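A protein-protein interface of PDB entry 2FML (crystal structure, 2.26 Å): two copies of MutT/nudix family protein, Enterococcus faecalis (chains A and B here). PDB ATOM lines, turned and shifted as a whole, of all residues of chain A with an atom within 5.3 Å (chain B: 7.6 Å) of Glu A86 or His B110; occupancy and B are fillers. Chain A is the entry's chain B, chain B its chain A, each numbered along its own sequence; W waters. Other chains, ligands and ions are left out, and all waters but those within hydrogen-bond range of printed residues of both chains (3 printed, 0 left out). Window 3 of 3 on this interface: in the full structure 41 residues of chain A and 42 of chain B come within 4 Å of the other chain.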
ATOM      1  N   SER A  84      38.806 -19.741  16.023  1.00  0.00           N
ATOM      2  CA  SER A  84      37.449 -20.277  15.883  1.00  0.00           C
ATOM      3  C   SER A  84      37.516 -21.633  15.211  1.00  0.00           C
ATOM      4  O   SER A  84      38.473 -21.929  14.531  1.00  0.00           O
ATOM      5  CB  SER A  84      36.598 -19.349  14.996  1.00  0.00           C
ATOM      6  OG  SER A  84      37.195 -19.295  13.731  1.00  0.00           O
ATOM      7  N   THR A  85      36.463 -22.433  15.348  1.00  0.00           N
ATOM      8  CA  THR A  85      36.368 -23.700  14.646  1.00  0.00           C
ATOM      9  C   THR A  85      36.415 -23.550  13.116  1.00  0.00           C
ATOM     10  O   THR A  85      36.944 -24.421  12.429  1.00  0.00           O
ATOM     11  CB  THR A  85      35.077 -24.499  15.082  1.00  0.00           C
ATOM     12  OG1 THR A  85      33.906 -23.794  14.655  1.00  0.00           O
ATOM     13  CG2 THR A  85      35.033 -24.656  16.622  1.00  0.00           C
ATOM     14  N   GLU A  86      35.843 -22.478  12.582  1.00  0.00           N
ATOM     15  CA  GLU A  86      35.970 -22.155  11.157  1.00  0.00           C
ATOM     16  C   GLU A  86      37.441 -22.028  10.820  1.00  0.00           C
ATOM     17  O   GLU A  86      37.858 -22.562   9.785  1.00  0.00           O
ATOM     18  CB  GLU A  86      35.295 -20.799  10.788  1.00  0.00           C
ATOM     19  CG  GLU A  86      33.740 -20.802  10.801  1.00  0.00           C
ATOM     20  CD  GLU A  86      33.101 -20.596  12.164  1.00  0.00           C
ATOM     21  OE1 GLU A  86      33.827 -20.293  13.150  1.00  0.00           O
ATOM     22  OE2 GLU A  86      31.855 -20.656  12.256  1.00  0.00           O
ATOM     23  N   ASP A  87      38.222 -21.262  11.615  1.00  0.00           N
ATOM     24  CA  ASP A  87      39.660 -21.202  11.368  1.00  0.00           C
ATOM     25  C   ASP A  87      40.321 -22.591  11.394  1.00  0.00           C
ATOM     26  O   ASP A  87      41.204 -22.831  10.581  1.00  0.00           O
ATOM     27  CB  ASP A  87      40.422 -20.348  12.385  1.00  0.00           C
ATOM     28  CG  ASP A  87      40.038 -18.863  12.357  1.00  0.00           C
ATOM     29  OD1 ASP A  87      39.537 -18.369  11.295  1.00  0.00           O
ATOM     30  OD2 ASP A  87      40.241 -18.221  13.451  1.00  0.00           O
ATOM     31  N   SER A  88      39.948 -23.447  12.351  1.00  0.00           N
ATOM     32  CA  SER A  88      40.585 -24.774  12.488  1.00  0.00           C
ATOM     33  C   SER A  88      40.297 -25.674  11.289  1.00  0.00           C
ATOM     34  O   SER A  88      41.201 -26.441  10.919  1.00  0.00           O
ATOM     35  CB  SER A  88      40.106 -25.493  13.774  1.00  0.00           C
ATOM     36  OG  SER A  88      40.230 -24.538  14.848  1.00  0.00           O
ATOM     37  N   VAL A  89      39.075 -25.576  10.703  1.00  0.00           N
ATOM     38  CA  VAL A  89      38.751 -26.316   9.515  1.00  0.00           C
ATOM     39  C   VAL A  89      39.707 -25.917   8.397  1.00  0.00           C
ATOM     40  O   VAL A  89      40.198 -26.765   7.705  1.00  0.00           O
ATOM     41  CB  VAL A  89      37.270 -26.035   9.062  1.00  0.00           C
ATOM     42  CG1 VAL A  89      36.920 -26.652   7.629  1.00  0.00           C
ATOM     43  CG2 VAL A  89      36.282 -26.531  10.104  1.00  0.00           C
ATOM     44  N   LEU A  90      39.938 -24.603   8.183  1.00  0.00           N
ATOM     45  CA  LEU A  90      40.755 -24.141   7.062  1.00  0.00           C
ATOM     46  C   LEU A  90      42.154 -24.714   7.280  1.00  0.00           C
ATOM     47  O   LEU A  90      42.757 -25.213   6.349  1.00  0.00           O
ATOM     48  CB  LEU A  90      40.798 -22.601   6.952  1.00  0.00           C
ATOM     49  CG  LEU A  90      39.503 -21.778   6.768  1.00  0.00           C
ATOM     50  CD1 LEU A  90      39.738 -20.242   6.318  1.00  0.00           C
ATOM     51  CD2 LEU A  90      38.497 -22.460   5.899  1.00  0.00           C
ATOM     52  N   GLN A 103      36.462 -19.828   4.083  1.00  0.00           N
ATOM     53  CA  GLN A 103      35.124 -20.025   4.643  1.00  0.00           C
ATOM     54  C   GLN A 103      33.969 -20.024   3.619  1.00  0.00           C
ATOM     55  O   GLN A 103      32.896 -20.543   3.922  1.00  0.00           O
ATOM     56  CB  GLN A 103      34.849 -18.963   5.704  1.00  0.00           C
ATOM     57  CG  GLN A 103      35.630 -19.289   7.021  1.00  0.00           C
ATOM     58  CD  GLN A 103      35.340 -18.333   8.131  1.00  0.00           C
ATOM     59  OE1 GLN A 103      36.248 -17.895   8.837  1.00  0.00           O
ATOM     60  NE2 GLN A 103      34.064 -18.029   8.331  1.00  0.00           N
ATOM     61  N   ILE A 106      33.063 -23.635   3.118  1.00  0.00           N
ATOM     62  CA  ILE A 106      32.650 -24.512   4.205  1.00  0.00           C
ATOM     63  C   ILE A 106      31.245 -24.241   4.724  1.00  0.00           C
ATOM     64  O   ILE A 106      30.703 -23.190   4.529  1.00  0.00           O
ATOM     65  CB  ILE A 106      33.694 -24.433   5.400  1.00  0.00           C
ATOM     66  CG1 ILE A 106      33.460 -23.154   6.239  1.00  0.00           C
ATOM     67  CG2 ILE A 106      35.082 -24.542   4.871  1.00  0.00           C
ATOM     68  CD1 ILE A 106      34.433 -23.023   7.455  1.00  0.00           C
ATOM     69  N   GLN A 108      29.251 -24.977   8.486  1.00  0.00           N
ATOM     70  CA  GLN A 108      29.077 -25.621   9.811  1.00  0.00           C
ATOM     71  C   GLN A 108      27.804 -26.500   9.789  1.00  0.00           C
ATOM     72  O   GLN A 108      26.719 -26.077   9.333  1.00  0.00           O
ATOM     73  CB  GLN A 108      29.024 -24.583  10.928  1.00  0.00           C
ATOM     74  CG  GLN A 108      29.224 -25.211  12.260  1.00  0.00           C
ATOM     75  CD  GLN A 108      29.006 -24.264  13.331  1.00  0.00           C
ATOM     76  OE1 GLN A 108      29.916 -23.422  13.726  1.00  0.00           O
ATOM     77  NE2 GLN A 108      27.795 -24.338  13.869  1.00  0.00           N
ATOM     78  N   TYR A 128      31.715 -29.959  10.076  1.00  0.00           N
ATOM     79  CA  TYR A 128      31.613 -29.049   8.949  1.00  0.00           C
ATOM     80  C   TYR A 128      31.574 -29.883   7.673  1.00  0.00           C
ATOM     81  O   TYR A 128      32.278 -30.936   7.569  1.00  0.00           O
ATOM     82  CB  TYR A 128      32.849 -28.121   8.838  1.00  0.00           C
ATOM     83  CG  TYR A 128      32.843 -26.942   9.783  1.00  0.00           C
ATOM     84  CD1 TYR A 128      33.110 -27.102  11.183  1.00  0.00           C
ATOM     85  CD2 TYR A 128      32.545 -25.671   9.316  1.00  0.00           C
ATOM     86  CE1 TYR A 128      33.062 -26.006  12.081  1.00  0.00           C
ATOM     87  CE2 TYR A 128      32.534 -24.549  10.213  1.00  0.00           C
ATOM     88  CZ  TYR A 128      32.782 -24.727  11.575  1.00  0.00           C
ATOM     89  OH  TYR A 128      32.728 -23.595  12.413  1.00  0.00           O
ATOM     90  N   ASP B  43      23.101 -21.898  24.567  1.00  0.00           N
ATOM     91  CA  ASP B  43      22.222 -20.762  24.659  1.00  0.00           C
ATOM     92  C   ASP B  43      20.988 -21.120  23.836  1.00  0.00           C
ATOM     93  O   ASP B  43      21.065 -21.875  22.812  1.00  0.00           O
ATOM     94  CB  ASP B  43      22.902 -19.511  24.048  1.00  0.00           C
ATOM     95  CG  ASP B  43      23.874 -18.847  25.025  1.00  0.00           C
ATOM     96  OD1 ASP B  43      23.392 -18.176  25.974  1.00  0.00           O
ATOM     97  OD2 ASP B  43      25.119 -19.028  24.875  1.00  0.00           O
ATOM     98  N   GLU B 107      15.860 -27.328  17.735  1.00  0.00           N
ATOM     99  CA  GLU B 107      16.844 -27.627  16.734  1.00  0.00           C
ATOM    100  C   GLU B 107      18.169 -26.936  17.069  1.00  0.00           C
ATOM    101  O   GLU B 107      18.183 -25.793  17.495  1.00  0.00           O
ATOM    102  CB  GLU B 107      16.344 -27.239  15.305  1.00  0.00           C
ATOM    103  CG  GLU B 107      16.261 -25.692  15.022  1.00  0.00           C
ATOM    104  CD  GLU B 107      15.499 -25.354  13.684  1.00  0.00           C
ATOM    105  OE1 GLU B 107      14.238 -25.492  13.666  1.00  0.00           O
ATOM    106  OE2 GLU B 107      16.168 -24.970  12.674  1.00  0.00           O
ATOM    107  N   GLN B 108      19.271 -27.615  16.804  1.00  0.00           N
ATOM    108  CA  GLN B 108      20.562 -26.976  16.974  1.00  0.00           C
ATOM    109  C   GLN B 108      20.720 -25.852  15.944  1.00  0.00           C
ATOM    110  O   GLN B 108      20.349 -26.012  14.787  1.00  0.00           O
ATOM    111  CB  GLN B 108      21.682 -27.995  16.891  1.00  0.00           C
ATOM    112  CG  GLN B 108      22.839 -27.610  17.671  1.00  0.00           C
ATOM    113  CD  GLN B 108      23.895 -28.652  17.600  1.00  0.00           C
ATOM    114  OE1 GLN B 108      23.974 -29.587  18.441  1.00  0.00           O
ATOM    115  NE2 GLN B 108      24.774 -28.477  16.649  1.00  0.00           N
ATOM    116  N   LEU B 109      21.182 -24.674  16.370  1.00  0.00           N
ATOM    117  CA  LEU B 109      21.183 -23.568  15.434  1.00  0.00           C
ATOM    118  C   LEU B 109      22.609 -23.367  14.834  1.00  0.00           C
ATOM    119  O   LEU B 109      22.812 -23.413  13.603  1.00  0.00           O
ATOM    120  CB  LEU B 109      20.643 -22.302  16.130  1.00  0.00           C
ATOM    121  CG  LEU B 109      20.802 -20.916  15.469  1.00  0.00           C
ATOM    122  CD1 LEU B 109      20.078 -20.815  14.145  1.00  0.00           C
ATOM    123  CD2 LEU B 109      20.375 -19.811  16.441  1.00  0.00           C
ATOM    124  N   HIS B 110      23.583 -23.129  15.711  1.00  0.00           N
ATOM    125  CA  HIS B 110      24.914 -22.784  15.304  1.00  0.00           C
ATOM    126  C   HIS B 110      25.823 -22.777  16.559  1.00  0.00           C
ATOM    127  O   HIS B 110      25.343 -22.477  17.684  1.00  0.00           O
ATOM    128  CB  HIS B 110      24.922 -21.429  14.602  1.00  0.00           C
ATOM    129  CG  HIS B 110      26.257 -21.060  14.033  1.00  0.00           C
ATOM    130  ND1 HIS B 110      26.689 -21.455  12.773  1.00  0.00           N
ATOM    131  CD2 HIS B 110      27.258 -20.311  14.555  1.00  0.00           C
ATOM    132  CE1 HIS B 110      27.903 -20.965  12.557  1.00  0.00           C
ATOM    133  NE2 HIS B 110      28.268 -20.272  13.629  1.00  0.00           N
ATOM    134  N   SER B 111      27.107 -23.130  16.376  1.00  0.00           N
ATOM    135  CA  SER B 111      28.084 -23.019  17.434  1.00  0.00           C
ATOM    136  C   SER B 111      28.966 -21.820  17.151  1.00  0.00           C
ATOM    137  O   SER B 111      29.532 -21.722  16.077  1.00  0.00           O
ATOM    138  CB  SER B 111      28.957 -24.247  17.590  1.00  0.00           C
ATOM    139  OG  SER B 111      28.106 -25.349  17.466  1.00  0.00           O
ATOM    140  N   PHE B 112      29.125 -21.005  18.198  1.00  0.00           N
ATOM    141  CA  PHE B 112      29.908 -19.783  18.207  1.00  0.00           C
ATOM    142  C   PHE B 112      31.142 -19.955  19.028  1.00  0.00           C
ATOM    143  O   PHE B 112      31.073 -20.419  20.176  1.00  0.00           O
ATOM    144  CB  PHE B 112      29.019 -18.692  18.790  1.00  0.00           C
ATOM    145  CG  PHE B 112      27.860 -18.362  17.886  1.00  0.00           C
ATOM    146  CD1 PHE B 112      27.979 -17.366  16.917  1.00  0.00           C
ATOM    147  CD2 PHE B 112      26.649 -19.028  18.050  1.00  0.00           C
ATOM    148  CE1 PHE B 112      26.895 -17.088  16.079  1.00  0.00           C
ATOM    149  CE2 PHE B 112      25.591 -18.755  17.229  1.00  0.00           C
ATOM    150  CZ  PHE B 112      25.709 -17.821  16.236  1.00  0.00           C
ATOM    151  N   SER B 113      32.277 -19.647  18.401  1.00  0.00           N
ATOM    152  CA  SER B 113      33.550 -20.010  18.905  1.00  0.00           C
ATOM    153  C   SER B 113      34.606 -18.937  18.733  1.00  0.00           C
ATOM    154  O   SER B 113      35.805 -19.209  18.913  1.00  0.00           O
ATOM    155  CB  SER B 113      34.018 -21.267  18.223  1.00  0.00           C
ATOM    156  OG  SER B 113      34.154 -21.050  16.802  1.00  0.00           O
ATOM    157  N   ARG B 114      34.180 -17.746  18.395  1.00  0.00           N
ATOM    158  CA  ARG B 114      35.117 -16.655  18.247  1.00  0.00           C
ATOM    159  C   ARG B 114      35.932 -16.563  19.560  1.00  0.00           C
ATOM    160  O   ARG B 114      35.359 -16.638  20.639  1.00  0.00           O
ATOM    161  CB  ARG B 114      34.338 -15.357  18.033  1.00  0.00           C
ATOM    162  CG  ARG B 114      35.164 -14.172  18.403  1.00  0.00           C
ATOM    163  CD  ARG B 114      34.611 -12.930  17.618  1.00  0.00           C
ATOM    164  NE  ARG B 114      33.267 -12.554  18.098  1.00  0.00           N
ATOM    165  CZ  ARG B 114      33.069 -11.832  19.187  1.00  0.00           C
ATOM    166  NH1 ARG B 114      34.118 -11.405  19.930  1.00  0.00           N
ATOM    167  NH2 ARG B 114      31.850 -11.499  19.484  1.00  0.00           N
ATOM    168  N   THR B 125      29.945 -21.829  22.630  1.00  0.00           N
ATOM    169  CA  THR B 125      28.568 -22.057  22.846  1.00  0.00           C
ATOM    170  C   THR B 125      27.880 -22.807  21.673  1.00  0.00           C
ATOM    171  O   THR B 125      28.157 -22.582  20.537  1.00  0.00           O
ATOM    172  CB  THR B 125      27.912 -20.738  23.249  1.00  0.00           C
ATOM    173  OG1 THR B 125      26.754 -21.006  24.038  1.00  0.00           O
ATOM    174  CG2 THR B 125      27.498 -19.871  22.012  1.00  0.00           C
ATOM    175  N   VAL B 126      27.007 -23.737  21.986  1.00  0.00           N
ATOM    176  CA  VAL B 126      26.208 -24.360  21.006  1.00  0.00           C
ATOM    177  C   VAL B 126      24.836 -23.730  21.215  1.00  0.00           C
ATOM    178  O   VAL B 126      24.220 -23.862  22.253  1.00  0.00           O
ATOM    179  CB  VAL B 126      26.181 -25.869  21.167  1.00  0.00           C
ATOM    180  CG1 VAL B 126      25.312 -26.488  20.141  1.00  0.00           C
ATOM    181  CG2 VAL B 126      27.552 -26.412  21.114  1.00  0.00           C
ATOM    182  N   SER B 127      24.409 -22.952  20.262  1.00  0.00           N
ATOM    183  CA  SER B 127      23.085 -22.374  20.375  1.00  0.00           C
ATOM    184  C   SER B 127      21.979 -23.278  19.740  1.00  0.00           C
ATOM    185  O   SER B 127      22.223 -24.036  18.828  1.00  0.00           O
ATOM    186  CB  SER B 127      23.059 -20.950  19.792  1.00  0.00           C
ATOM    187  OG  SER B 127      23.206 -20.974  18.378  1.00  0.00           O
ATOM    188  N   TYR B 128      20.782 -23.130  20.283  1.00  0.00           N
ATOM    189  CA  TYR B 128      19.578 -23.812  19.864  1.00  0.00           C
ATOM    190  C   TYR B 128      18.433 -22.828  19.607  1.00  0.00           C
ATOM    191  O   TYR B 128      18.420 -21.742  20.146  1.00  0.00           O
ATOM    192  CB  TYR B 128      19.156 -24.844  20.928  1.00  0.00           C
ATOM    193  CG  TYR B 128      20.048 -26.047  20.954  1.00  0.00           C
ATOM    194  CD1 TYR B 128      19.632 -27.242  20.383  1.00  0.00           C
ATOM    195  CD2 TYR B 128      21.310 -26.005  21.637  1.00  0.00           C
ATOM    196  CE1 TYR B 128      20.440 -28.390  20.464  1.00  0.00           C
ATOM    197  CE2 TYR B 128      22.109 -27.108  21.732  1.00  0.00           C
ATOM    198  CZ  TYR B 128      21.700 -28.280  21.105  1.00  0.00           C
ATOM    199  OH  TYR B 128      22.522 -29.342  21.147  1.00  0.00           O
ATOM    200  N   LEU B 129      17.462 -23.292  18.823  1.00  0.00           N
ATOM    201  CA  LEU B 129      16.270 -22.551  18.403  1.00  0.00           C
ATOM    202  C   LEU B 129      15.042 -23.435  18.713  1.00  0.00           C
ATOM    203  O   LEU B 129      15.059 -24.641  18.489  1.00  0.00           O
ATOM    204  CB  LEU B 129      16.341 -22.308  16.895  1.00  0.00           C
ATOM    205  CG  LEU B 129      15.176 -21.697  16.118  1.00  0.00           C
ATOM    206  CD1 LEU B 129      14.649 -20.399  16.837  1.00  0.00           C
ATOM    207  CD2 LEU B 129      15.678 -21.349  14.708  1.00  0.00           C
ATOM    208  N   GLU B 188      24.533 -11.582  17.578  1.00  0.00           N
ATOM    209  CA  GLU B 188      24.839 -12.469  16.461  1.00  0.00           C
ATOM    210  C   GLU B 188      24.040 -13.738  16.452  1.00  0.00           C
ATOM    211  O   GLU B 188      23.822 -14.302  15.419  1.00  0.00           O
ATOM    212  CB  GLU B 188      26.328 -12.905  16.406  1.00  0.00           C
ATOM    213  CG  GLU B 188      27.298 -11.843  15.987  1.00  0.00           C
ATOM    214  CD  GLU B 188      28.681 -12.231  16.419  1.00  0.00           C
ATOM    215  OE1 GLU B 188      29.074 -13.335  15.998  1.00  0.00           O
ATOM    216  OE2 GLU B 188      29.339 -11.479  17.215  1.00  0.00           O
ATOM    217  N   ILE B 189      23.803 -14.271  17.633  1.00  0.00           N
ATOM    218  CA  ILE B 189      23.022 -15.458  17.791  1.00  0.00           C
ATOM    219  C   ILE B 189      21.517 -15.209  17.447  1.00  0.00           C
ATOM    220  O   ILE B 189      20.895 -16.039  16.788  1.00  0.00           O
ATOM    221  CB  ILE B 189      23.152 -16.071  19.232  1.00  0.00           C
ATOM    222  CG1 ILE B 189      24.621 -16.158  19.769  1.00  0.00           C
ATOM    223  CG2 ILE B 189      22.355 -17.363  19.286  1.00  0.00           C
ATOM    224  CD1 ILE B 189      24.735 -16.982  21.113  1.00  0.00           C
ATOM    225  N   LYS B 192      21.342 -14.808  13.708  1.00  0.00           N
ATOM    226  CA  LYS B 192      21.461 -16.176  13.103  1.00  0.00           C
ATOM    227  C   LYS B 192      20.131 -16.942  13.145  1.00  0.00           C
ATOM    228  O   LYS B 192      19.725 -17.537  12.148  1.00  0.00           O
ATOM    229  CB  LYS B 192      22.597 -16.993  13.735  1.00  0.00           C
ATOM    230  CG  LYS B 192      23.007 -18.348  13.051  1.00  0.00           C
ATOM    231  CD  LYS B 192      23.982 -18.238  11.811  1.00  0.00           C
ATOM    232  CE  LYS B 192      25.382 -17.718  12.067  1.00  0.00           C
ATOM    233  NZ  LYS B 192      26.254 -17.836  10.739  1.00  0.00           N
ATOM    234  N   ALA B 193      19.461 -16.903  14.290  1.00  0.00           N
ATOM    235  CA  ALA B 193      18.157 -17.561  14.481  1.00  0.00           C
ATOM    236  C   ALA B 193      17.096 -16.968  13.582  1.00  0.00           C
ATOM    237  O   ALA B 193      16.287 -17.729  12.964  1.00  0.00           O
ATOM    238  CB  ALA B 193      17.713 -17.497  15.980  1.00  0.00           C
ATOM    239  N   ARG B 196      17.820 -17.825   9.931  1.00  0.00           N
ATOM    240  CA  ARG B 196      17.662 -19.261   9.713  1.00  0.00           C
ATOM    241  C   ARG B 196      16.208 -19.601   9.418  1.00  0.00           C
ATOM    242  O   ARG B 196      15.933 -20.422   8.544  1.00  0.00           O
ATOM    243  CB  ARG B 196      18.187 -20.095  10.911  1.00  0.00           C
ATOM    244  CG  ARG B 196      17.894 -21.635  10.811  1.00  0.00           C
ATOM    245  CD  ARG B 196      18.844 -22.310   9.814  1.00  0.00           C
ATOM    246  NE  ARG B 196      20.186 -21.673   9.871  1.00  0.00           N
ATOM    247  CZ  ARG B 196      21.228 -22.105  10.555  1.00  0.00           C
ATOM    248  NH1 ARG B 196      21.142 -23.231  11.272  1.00  0.00           N
ATOM    249  NH2 ARG B 196      22.371 -21.416  10.502  1.00  0.00           N
HETATM  250  O   HOH W   1      25.908 -26.223  15.803  1.00  0.00           O
HETATM  251  O   HOH W   2      30.353 -18.693  13.762  1.00  0.00           O
HETATM  252  O   HOH W   3      32.135 -20.912  15.165  1.00  0.00           O
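The side-chain amide nitrogen (NE2) of Gln A108 lies close to the backbone NH (N) of Ser B111, 2.9 Å away.
The side-chain hydroxyl of Ser B113 lies within hydrogen-bond range of the backbone NH of Thr A85, at 3.1 Å.
A ring nitrogen (ND1) of His B110 sits at hydrogen-bond distance from the side-chain amide nitrogen (NE2) of Gln A108, 3.3 Å away.
The side-chain hydroxyl of Tyr A128 lies close to the side-chain carboxylate of Glu A86 (3.1 Å).
OG of Ser A84 lies within hydrogen-bond range of N of Asp A87.
O of Ser A84 lies within hydrogen-bond range of OG of Ser A88.
O of His B110 is in hydrogen-bond range of OG of Ser B127, 2.7 Å away.
The side-chain amide oxygen (OE1) of Gln A108 sits at hydrogen-bond distance from the side-chain hydroxyl (OH) of Tyr A128.
OG1 of Thr A85 is in hydrogen-bond range of OH of Tyr A128 (2.5 Å).
Water W3 lies within hydrogen-bond range of the side-chain hydroxyl (OG) of Ser B113 (2.6 Å), the side-chain carboxylate (OE1) of Glu A86 (2.7 Å), the backbone carbonyl oxygen (O) of Ser B111 (2.9 Å) and the side-chain hydroxyl (OG1) of Thr A85 (3.4 Å).
Water W2 lies within hydrogen-bond range of NE2 of His B110 (2.6 Å) and OE2 of Glu A86 (2.9 Å).
Water W1 lies within hydrogen-bond range of NE2 of Gln B108 (2.7 Å), OG of Ser B111 (2.9 Å) and NE2 of Gln A108 (3.3 Å).
Among the printed residues, pairs that only touch across the chains: Ser A84 with Ser B113 (3.5 Å), Glu A86 with His B110 (3.9 Å) and Glu A86 with Ser B113 (3.7 Å).
Of the printed residues of chain B, Ser A84 touches Ser B113.
Printed residues of chain B within 4 Å of Thr A85: Ser B113 (3.1 Å).
Of the printed residues of chain B, Glu A86 touches His B110 (3.9 Å) and Ser B113 (3.7 Å).
Of the printed residues of chain B, Gln A108 touches His B110 and Ser B111.
His B110 touches two residues of chain A.
Of the printed residues of chain A, Ser B111 touches Gln A108 (2.9 Å).
The nearest printed residue of chain A that does not touch His B110 is Tyr A128 (5.5 Å).
The nearest printed residue of chain B that does not touch Ser A84 is Arg B114 (4.5 Å).
2 positions are printed for both chains.
Of the 6 pairs that touch across the chains among the printed residues, none has its exchanged pair printed and touching as well.
Hydrophobic or aromatic side chains of chain B that line the printed part of chain A: His B110.
Among the printed residues, 6 pairs touch across the chains.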
